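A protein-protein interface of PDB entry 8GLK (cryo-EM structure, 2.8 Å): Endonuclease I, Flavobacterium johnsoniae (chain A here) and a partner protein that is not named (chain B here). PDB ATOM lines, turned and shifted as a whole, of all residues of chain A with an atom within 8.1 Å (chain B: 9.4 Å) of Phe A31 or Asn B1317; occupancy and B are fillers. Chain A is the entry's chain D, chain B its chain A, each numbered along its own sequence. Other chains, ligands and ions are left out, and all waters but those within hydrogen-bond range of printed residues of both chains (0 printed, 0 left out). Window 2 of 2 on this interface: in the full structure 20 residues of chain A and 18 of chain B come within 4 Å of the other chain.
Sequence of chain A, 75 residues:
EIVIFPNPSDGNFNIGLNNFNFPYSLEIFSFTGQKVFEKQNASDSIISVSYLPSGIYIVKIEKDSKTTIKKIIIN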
ATOM      1  N   ILE A  28     -15.195   7.713  -1.694  1.00  0.00           N
ATOM      2  CA  ILE A  28     -15.497   6.288  -1.625  1.00  0.00           C
ATOM      3  C   ILE A  28     -16.441   5.937  -2.765  1.00  0.00           C
ATOM      4  O   ILE A  28     -17.496   6.565  -2.929  1.00  0.00           O
ATOM      5  CB  ILE A  28     -16.101   5.902  -0.265  1.00  0.00           C
ATOM      6  CG1 ILE A  28     -15.090   6.137   0.855  1.00  0.00           C
ATOM      7  CG2 ILE A  28     -16.550   4.449  -0.272  1.00  0.00           C
ATOM      8  CD1 ILE A  28     -15.626   5.835   2.236  1.00  0.00           C
ATOM      9  N   PHE A  29     -16.054   4.921  -3.535  1.00  0.00           N
ATOM     10  CA  PHE A  29     -16.725   4.479  -4.745  1.00  0.00           C
ATOM     11  C   PHE A  29     -17.200   3.044  -4.563  1.00  0.00           C
ATOM     12  O   PHE A  29     -16.504   2.218  -3.966  1.00  0.00           O
ATOM     13  CB  PHE A  29     -15.771   4.532  -5.940  1.00  0.00           C
ATOM     14  CG  PHE A  29     -15.146   5.876  -6.168  1.00  0.00           C
ATOM     15  CD1 PHE A  29     -15.768   6.825  -6.958  1.00  0.00           C
ATOM     16  CD2 PHE A  29     -13.895   6.165  -5.644  1.00  0.00           C
ATOM     17  CE1 PHE A  29     -15.172   8.050  -7.189  1.00  0.00           C
ATOM     18  CE2 PHE A  29     -13.301   7.390  -5.864  1.00  0.00           C
ATOM     19  CZ  PHE A  29     -13.940   8.333  -6.638  1.00  0.00           C
ATOM     20  N   SER A  30     -18.379   2.748  -5.100  1.00  0.00           N
ATOM     21  CA  SER A  30     -18.907   1.394  -5.088  1.00  0.00           C
ATOM     22  C   SER A  30     -18.321   0.584  -6.243  1.00  0.00           C
ATOM     23  O   SER A  30     -17.652   1.113  -7.132  1.00  0.00           O
ATOM     24  CB  SER A  30     -20.432   1.411  -5.170  1.00  0.00           C
ATOM     25  OG  SER A  30     -20.867   1.963  -6.399  1.00  0.00           O
ATOM     26  N   PHE A  31     -18.580  -0.727  -6.218  1.00  0.00           N
ATOM     27  CA  PHE A  31     -18.123  -1.580  -7.310  1.00  0.00           C
ATOM     28  C   PHE A  31     -18.807  -1.221  -8.622  1.00  0.00           C
ATOM     29  O   PHE A  31     -18.272  -1.511  -9.698  1.00  0.00           O
ATOM     30  CB  PHE A  31     -18.365  -3.053  -6.981  1.00  0.00           C
ATOM     31  CG  PHE A  31     -17.816  -3.998  -8.014  1.00  0.00           C
ATOM     32  CD1 PHE A  31     -16.479  -4.356  -8.001  1.00  0.00           C
ATOM     33  CD2 PHE A  31     -18.630  -4.511  -9.010  1.00  0.00           C
ATOM     34  CE1 PHE A  31     -15.969  -5.219  -8.951  1.00  0.00           C
ATOM     35  CE2 PHE A  31     -18.126  -5.374  -9.964  1.00  0.00           C
ATOM     36  CZ  PHE A  31     -16.794  -5.729  -9.934  1.00  0.00           C
ATOM     37  N   THR A  32     -19.988  -0.606  -8.557  1.00  0.00           N
ATOM     38  CA  THR A  32     -20.657  -0.146  -9.767  1.00  0.00           C
ATOM     39  C   THR A  32     -19.963   1.059 -10.384  1.00  0.00           C
ATOM     40  O   THR A  32     -20.312   1.455 -11.501  1.00  0.00           O
ATOM     41  CB  THR A  32     -22.115   0.207  -9.463  1.00  0.00           C
ATOM     42  OG1 THR A  32     -22.159   1.261  -8.493  1.00  0.00           O
ATOM     43  CG2 THR A  32     -22.852  -1.001  -8.917  1.00  0.00           C
ATOM     44  N   GLY A  33     -18.992   1.645  -9.688  1.00  0.00           N
ATOM     45  CA  GLY A  33     -18.393   2.892 -10.099  1.00  0.00           C
ATOM     46  C   GLY A  33     -19.128   4.121  -9.617  1.00  0.00           C
ATOM     47  O   GLY A  33     -18.660   5.239  -9.863  1.00  0.00           O
ATOM     48  N   GLN A  34     -20.257   3.949  -8.939  1.00  0.00           N
ATOM     49  CA  GLN A  34     -21.048   5.079  -8.478  1.00  0.00           C
ATOM     50  C   GLN A  34     -20.341   5.810  -7.345  1.00  0.00           C
ATOM     51  O   GLN A  34     -19.588   5.214  -6.569  1.00  0.00           O
ATOM     52  CB  GLN A  34     -22.424   4.601  -8.016  1.00  0.00           C
ATOM     53  CG  GLN A  34     -23.417   5.709  -7.722  1.00  0.00           C
ATOM     54  CD  GLN A  34     -24.731   5.182  -7.180  1.00  0.00           C
ATOM     55  OE1 GLN A  34     -24.839   4.009  -6.819  1.00  0.00           O
ATOM     56  NE2 GLN A  34     -25.737   6.046  -7.123  1.00  0.00           N
ATOM     57  N   VAL A  36     -20.434   7.138  -3.872  1.00  0.00           N
ATOM     58  CA  VAL A  36     -21.246   6.826  -2.704  1.00  0.00           C
ATOM     59  C   VAL A  36     -20.802   7.648  -1.502  1.00  0.00           C
ATOM     60  O   VAL A  36     -21.568   7.812  -0.545  1.00  0.00           O
ATOM     61  CB  VAL A  36     -21.222   5.317  -2.387  1.00  0.00           C
ATOM     62  CG1 VAL A  36     -21.641   4.514  -3.609  1.00  0.00           C
ATOM     63  CG2 VAL A  36     -19.857   4.887  -1.894  1.00  0.00           C
ATOM     64  N   SER A  54     -23.160  -4.088   1.742  1.00  0.00           N
ATOM     65  CA  SER A  54     -21.916  -4.832   1.879  1.00  0.00           C
ATOM     66  C   SER A  54     -21.248  -5.042   0.523  1.00  0.00           C
ATOM     67  O   SER A  54     -21.908  -5.120  -0.516  1.00  0.00           O
ATOM     68  CB  SER A  54     -22.179  -6.182   2.545  1.00  0.00           C
ATOM     69  OG  SER A  54     -22.685  -6.013   3.857  1.00  0.00           O
ATOM     70  N   GLY A  55     -19.931  -5.133   0.545  1.00  0.00           N
ATOM     71  CA  GLY A  55     -19.161  -5.348  -0.666  1.00  0.00           C
ATOM     72  C   GLY A  55     -17.808  -4.678  -0.560  1.00  0.00           C
ATOM     73  O   GLY A  55     -17.430  -4.142   0.475  1.00  0.00           O
ATOM     74  N   ILE A  56     -17.076  -4.726  -1.663  1.00  0.00           N
ATOM     75  CA  ILE A  56     -15.784  -4.056  -1.742  1.00  0.00           C
ATOM     76  C   ILE A  56     -15.998  -2.638  -2.244  1.00  0.00           C
ATOM     77  O   ILE A  56     -16.874  -2.377  -3.079  1.00  0.00           O
ATOM     78  CB  ILE A  56     -14.801  -4.832  -2.641  1.00  0.00           C
ATOM     79  CG1 ILE A  56     -15.222  -4.748  -4.108  1.00  0.00           C
ATOM     80  CG2 ILE A  56     -14.695  -6.280  -2.189  1.00  0.00           C
ATOM     81  CD1 ILE A  56     -14.081  -4.951  -5.070  1.00  0.00           C
ATOM     82  N   TYR A  57     -15.210  -1.709  -1.714  1.00  0.00           N
ATOM     83  CA  TYR A  57     -15.305  -0.304  -2.074  1.00  0.00           C
ATOM     84  C   TYR A  57     -13.913   0.248  -2.332  1.00  0.00           C
ATOM     85  O   TYR A  57     -12.919  -0.241  -1.788  1.00  0.00           O
ATOM     86  CB  TYR A  57     -16.006   0.508  -0.979  1.00  0.00           C
ATOM     87  CG  TYR A  57     -17.484   0.215  -0.873  1.00  0.00           C
ATOM     88  CD1 TYR A  57     -17.954  -0.798  -0.048  1.00  0.00           C
ATOM     89  CD2 TYR A  57     -18.409   0.941  -1.609  1.00  0.00           C
ATOM     90  CE1 TYR A  57     -19.304  -1.072   0.047  1.00  0.00           C
ATOM     91  CE2 TYR A  57     -19.760   0.675  -1.521  1.00  0.00           C
ATOM     92  CZ  TYR A  57     -20.203  -0.333  -0.692  1.00  0.00           C
ATOM     93  OH  TYR A  57     -21.548  -0.601  -0.602  1.00  0.00           O
ATOM     94  N   ILE A  58     -13.850   1.270  -3.180  1.00  0.00           N
ATOM     95  CA  ILE A  58     -12.591   1.892  -3.572  1.00  0.00           C
ATOM     96  C   ILE A  58     -12.481   3.240  -2.879  1.00  0.00           C
ATOM     97  O   ILE A  58     -13.352   4.102  -3.038  1.00  0.00           O
ATOM     98  CB  ILE A  58     -12.498   2.046  -5.098  1.00  0.00           C
ATOM     99  CG1 ILE A  58     -12.392   0.675  -5.768  1.00  0.00           C
ATOM    100  CG2 ILE A  58     -11.309   2.914  -5.472  1.00  0.00           C
ATOM    101  CD1 ILE A  58     -11.228  -0.155  -5.278  1.00  0.00           C
ATOM    102  N   PHE B 784     -27.186   6.107 -12.416  1.00  0.00           N
ATOM    103  CA  PHE B 784     -26.881   4.779 -11.898  1.00  0.00           C
ATOM    104  C   PHE B 784     -28.151   4.033 -11.508  1.00  0.00           C
ATOM    105  O   PHE B 784     -28.298   2.841 -11.805  1.00  0.00           O
ATOM    106  CB  PHE B 784     -25.935   4.889 -10.704  1.00  0.00           C
ATOM    107  CG  PHE B 784     -24.583   5.442 -11.054  1.00  0.00           C
ATOM    108  CD1 PHE B 784     -23.577   4.610 -11.513  1.00  0.00           C
ATOM    109  CD2 PHE B 784     -24.321   6.795 -10.928  1.00  0.00           C
ATOM    110  CE1 PHE B 784     -22.335   5.116 -11.836  1.00  0.00           C
ATOM    111  CE2 PHE B 784     -23.080   7.307 -11.249  1.00  0.00           C
ATOM    112  CZ  PHE B 784     -22.087   6.467 -11.704  1.00  0.00           C
ATOM    113  N   ILE B 949     -28.245 -10.867  -1.368  1.00  0.00           N
ATOM    114  CA  ILE B 949     -26.834 -11.045  -1.045  1.00  0.00           C
ATOM    115  C   ILE B 949     -26.093 -11.411  -2.320  1.00  0.00           C
ATOM    116  O   ILE B 949     -26.537 -12.286  -3.074  1.00  0.00           O
ATOM    117  CB  ILE B 949     -26.633 -12.122   0.034  1.00  0.00           C
ATOM    118  CG1 ILE B 949     -27.317 -11.708   1.335  1.00  0.00           C
ATOM    119  CG2 ILE B 949     -25.152 -12.378   0.272  1.00  0.00           C
ATOM    120  CD1 ILE B 949     -27.142 -12.710   2.444  1.00  0.00           C
ATOM    121  N   ALA B 950     -24.973 -10.736  -2.566  1.00  0.00           N
ATOM    122  CA  ALA B 950     -24.138 -11.071  -3.710  1.00  0.00           C
ATOM    123  C   ALA B 950     -23.631 -12.501  -3.593  1.00  0.00           C
ATOM    124  O   ALA B 950     -23.257 -12.959  -2.509  1.00  0.00           O
ATOM    125  CB  ALA B 950     -22.964 -10.100  -3.811  1.00  0.00           C
ATOM    126  N   GLN B 951     -23.628 -13.212  -4.717  1.00  0.00           N
ATOM    127  CA  GLN B 951     -23.200 -14.602  -4.718  1.00  0.00           C
ATOM    128  C   GLN B 951     -21.715 -14.702  -4.389  1.00  0.00           C
ATOM    129  O   GLN B 951     -20.897 -13.925  -4.889  1.00  0.00           O
ATOM    130  CB  GLN B 951     -23.488 -15.244  -6.073  1.00  0.00           C
ATOM    131  CG  GLN B 951     -24.924 -15.076  -6.540  1.00  0.00           C
ATOM    132  CD  GLN B 951     -25.923 -15.777  -5.639  1.00  0.00           C
ATOM    133  OE1 GLN B 951     -25.587 -16.739  -4.948  1.00  0.00           O
ATOM    134  NE2 GLN B 951     -27.159 -15.294  -5.639  1.00  0.00           N
ATOM    135  N   GLY B 952     -21.372 -15.670  -3.543  1.00  0.00           N
ATOM    136  CA  GLY B 952     -20.020 -15.823  -3.056  1.00  0.00           C
ATOM    137  C   GLY B 952     -19.728 -15.106  -1.758  1.00  0.00           C
ATOM    138  O   GLY B 952     -18.632 -15.279  -1.208  1.00  0.00           O
ATOM    139  N   GLN B 953     -20.664 -14.313  -1.251  1.00  0.00           N
ATOM    140  CA  GLN B 953     -20.494 -13.579  -0.011  1.00  0.00           C
ATOM    141  C   GLN B 953     -21.088 -14.377   1.148  1.00  0.00           C
ATOM    142  O   GLN B 953     -21.457 -15.546   1.005  1.00  0.00           O
ATOM    143  CB  GLN B 953     -21.126 -12.191  -0.131  1.00  0.00           C
ATOM    144  CG  GLN B 953     -20.534 -11.338  -1.239  1.00  0.00           C
ATOM    145  CD  GLN B 953     -19.019 -11.358  -1.244  1.00  0.00           C
ATOM    146  OE1 GLN B 953     -18.395 -11.827  -2.196  1.00  0.00           O
ATOM    147  NE2 GLN B 953     -18.417 -10.850  -0.175  1.00  0.00           N
ATOM    148  N   LEU B1314     -28.900  -2.566  -8.375  1.00  0.00           N
ATOM    149  CA  LEU B1314     -27.487  -2.359  -8.654  1.00  0.00           C
ATOM    150  C   LEU B1314     -26.844  -3.697  -9.000  1.00  0.00           C
ATOM    151  O   LEU B1314     -27.486  -4.747  -8.955  1.00  0.00           O
ATOM    152  CB  LEU B1314     -26.776  -1.699  -7.466  1.00  0.00           C
ATOM    153  CG  LEU B1314     -27.151  -0.242  -7.197  1.00  0.00           C
ATOM    154  CD1 LEU B1314     -26.338   0.316  -6.041  1.00  0.00           C
ATOM    155  CD2 LEU B1314     -26.953   0.596  -8.450  1.00  0.00           C
ATOM    156  N   TYR B1315     -25.560  -3.654  -9.346  1.00  0.00           N
ATOM    157  CA  TYR B1315     -24.791  -4.846  -9.687  1.00  0.00           C
ATOM    158  C   TYR B1315     -23.646  -4.976  -8.693  1.00  0.00           C
ATOM    159  O   TYR B1315     -22.700  -4.183  -8.723  1.00  0.00           O
ATOM    160  CB  TYR B1315     -24.267  -4.767 -11.120  1.00  0.00           C
ATOM    161  CG  TYR B1315     -25.115  -5.512 -12.125  1.00  0.00           C
ATOM    162  CD1 TYR B1315     -25.026  -6.890 -12.251  1.00  0.00           C
ATOM    163  CD2 TYR B1315     -26.003  -4.835 -12.949  1.00  0.00           C
ATOM    164  CE1 TYR B1315     -25.799  -7.575 -13.167  1.00  0.00           C
ATOM    165  CE2 TYR B1315     -26.779  -5.511 -13.869  1.00  0.00           C
ATOM    166  CZ  TYR B1315     -26.674  -6.881 -13.973  1.00  0.00           C
ATOM    167  OH  TYR B1315     -27.445  -7.559 -14.889  1.00  0.00           O
ATOM    168  N   ASN B1316     -23.725  -5.976  -7.813  1.00  0.00           N
ATOM    169  CA  ASN B1316     -22.668  -6.168  -6.824  1.00  0.00           C
ATOM    170  C   ASN B1316     -21.486  -6.922  -7.423  1.00  0.00           C
ATOM    171  O   ASN B1316     -20.384  -6.378  -7.533  1.00  0.00           O
ATOM    172  CB  ASN B1316     -23.218  -6.907  -5.604  1.00  0.00           C
ATOM    173  CG  ASN B1316     -22.374  -6.693  -4.364  1.00  0.00           C
ATOM    174  OD1 ASN B1316     -21.230  -7.144  -4.293  1.00  0.00           O
ATOM    175  ND2 ASN B1316     -22.934  -6.004  -3.378  1.00  0.00           N
ATOM    176  N   ASN B1317     -21.703  -8.178  -7.821  1.00  0.00           N
ATOM    177  CA  ASN B1317     -20.728  -8.978  -8.576  1.00  0.00           C
ATOM    178  C   ASN B1317     -21.526  -9.807  -9.579  1.00  0.00           C
ATOM    179  O   ASN B1317     -21.926 -10.935  -9.283  1.00  0.00           O
ATOM    180  CB  ASN B1317     -19.889  -9.867  -7.662  1.00  0.00           C
ATOM    181  CG  ASN B1317     -18.680  -9.155  -7.085  1.00  0.00           C
ATOM    182  OD1 ASN B1317     -18.364  -8.029  -7.458  1.00  0.00           O
ATOM    183  ND2 ASN B1317     -17.996  -9.819  -6.161  1.00  0.00           N
ATOM    184  N   ASN B1318     -21.744  -9.243 -10.769  1.00  0.00           N
ATOM    185  CA  ASN B1318     -22.513  -9.892 -11.835  1.00  0.00           C
ATOM    186  C   ASN B1318     -23.900 -10.330 -11.366  1.00  0.00           C
ATOM    187  O   ASN B1318     -24.556 -11.146 -12.023  1.00  0.00           O
ATOM    188  CB  ASN B1318     -21.749 -11.084 -12.421  1.00  0.00           C
ATOM    189  CG  ASN B1318     -20.310 -10.748 -12.747  1.00  0.00           C
ATOM    190  OD1 ASN B1318     -20.030  -9.755 -13.419  1.00  0.00           O
ATOM    191  ND2 ASN B1318     -19.386 -11.570 -12.267  1.00  0.00           N
ATOM    192  N   THR B1319     -24.362  -9.802 -10.235  1.00  0.00           N
ATOM    193  CA  THR B1319     -25.653 -10.152  -9.665  1.00  0.00           C
ATOM    194  C   THR B1319     -26.468  -8.887  -9.448  1.00  0.00           C
ATOM    195  O   THR B1319     -25.921  -7.834  -9.104  1.00  0.00           O
ATOM    196  CB  THR B1319     -25.494 -10.927  -8.341  1.00  0.00           C
ATOM    197  OG1 THR B1319     -26.773 -11.397  -7.898  1.00  0.00           O
ATOM    198  CG2 THR B1319     -24.865 -10.057  -7.261  1.00  0.00           C
ATOM    199  N   VAL B1320     -27.773  -8.986  -9.678  1.00  0.00           N
ATOM    200  CA  VAL B1320     -28.666  -7.849  -9.491  1.00  0.00           C
ATOM    201  C   VAL B1320     -29.113  -7.820  -8.036  1.00  0.00           C
ATOM    202  O   VAL B1320     -29.765  -8.754  -7.555  1.00  0.00           O
ATOM    203  CB  VAL B1320     -29.870  -7.926 -10.440  1.00  0.00           C
ATOM    204  CG1 VAL B1320     -30.840  -6.791 -10.154  1.00  0.00           C
ATOM    205  CG2 VAL B1320     -29.407  -7.888 -11.885  1.00  0.00           C
ATOM    206  N   ILE B1321     -28.764  -6.747  -7.334  1.00  0.00           N
ATOM    207  CA  ILE B1321     -29.112  -6.558  -5.933  1.00  0.00           C
ATOM    208  C   ILE B1321     -30.187  -5.486  -5.859  1.00  0.00           C
ATOM    209  O   ILE B1321     -29.982  -4.356  -6.323  1.00  0.00           O
ATOM    210  CB  ILE B1321     -27.888  -6.168  -5.090  1.00  0.00           C
ATOM    211  CG1 ILE B1321     -26.818  -7.257  -5.165  1.00  0.00           C
ATOM    212  CG2 ILE B1321     -28.292  -5.916  -3.646  1.00  0.00           C
ATOM    213  CD1 ILE B1321     -27.249  -8.574  -4.573  1.00  0.00           C
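OG of Ser A30 is in hydrogen-bond range of OG1 of Thr A32 (2.6 Å). The backbone NH of Gln A34 is in hydrogen-bond range of the side-chain hydroxyl of Ser A30, at 3.3 Å. OG1 of Thr A32 lies close to N of Gln A34.
Among the printed residues, merely in contact across the chains: Phe A31 with Asn B1316 (3.0 Å), Thr A32 with Tyr B1315 (3.2 Å), Gln A34 with Phe B784 (3.5 Å) and Phe A31 with Asn B1317 (3.7 Å).
Of the 13 printed residues of chain A, 4 touch a printed residue of chain B. Along chain A the printed residues that touch a printed residue of chain B span positions 31 to 54. Of the 14 printed residues of chain B, 4 touch a printed residue of chain A. Hydrophobic or aromatic side chains of chain B that line the printed part of chain A: Phe B784.
Phe A31 touches two residues of chain B. No residue of chain B comes within 4 Å of Ser A30. Of the printed residues of chain A, Asn B1316 touches Phe A31 (3.0 Å) and Ser A54 (3.2 Å). Of the printed residues of chain B, Ser A54 touches Asn B1316. Printed residues of chain A within 4 Å of Phe B784: Gln A34. Printed residues of chain A within 4 Å of Tyr B1315: Thr A32. The nearest residue of chain B that does not touch Phe A31 is Tyr B1315 (4.1 Å). The nearest printed residue of chain A that does not touch Tyr B1315 is Phe A31 (4.1 Å).
The backbone carbonyl oxygen (O) of Ser A54 lies within hydrogen-bond range of the side-chain amide nitrogen (ND2) of Asn B1316, at 3.2 Å.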
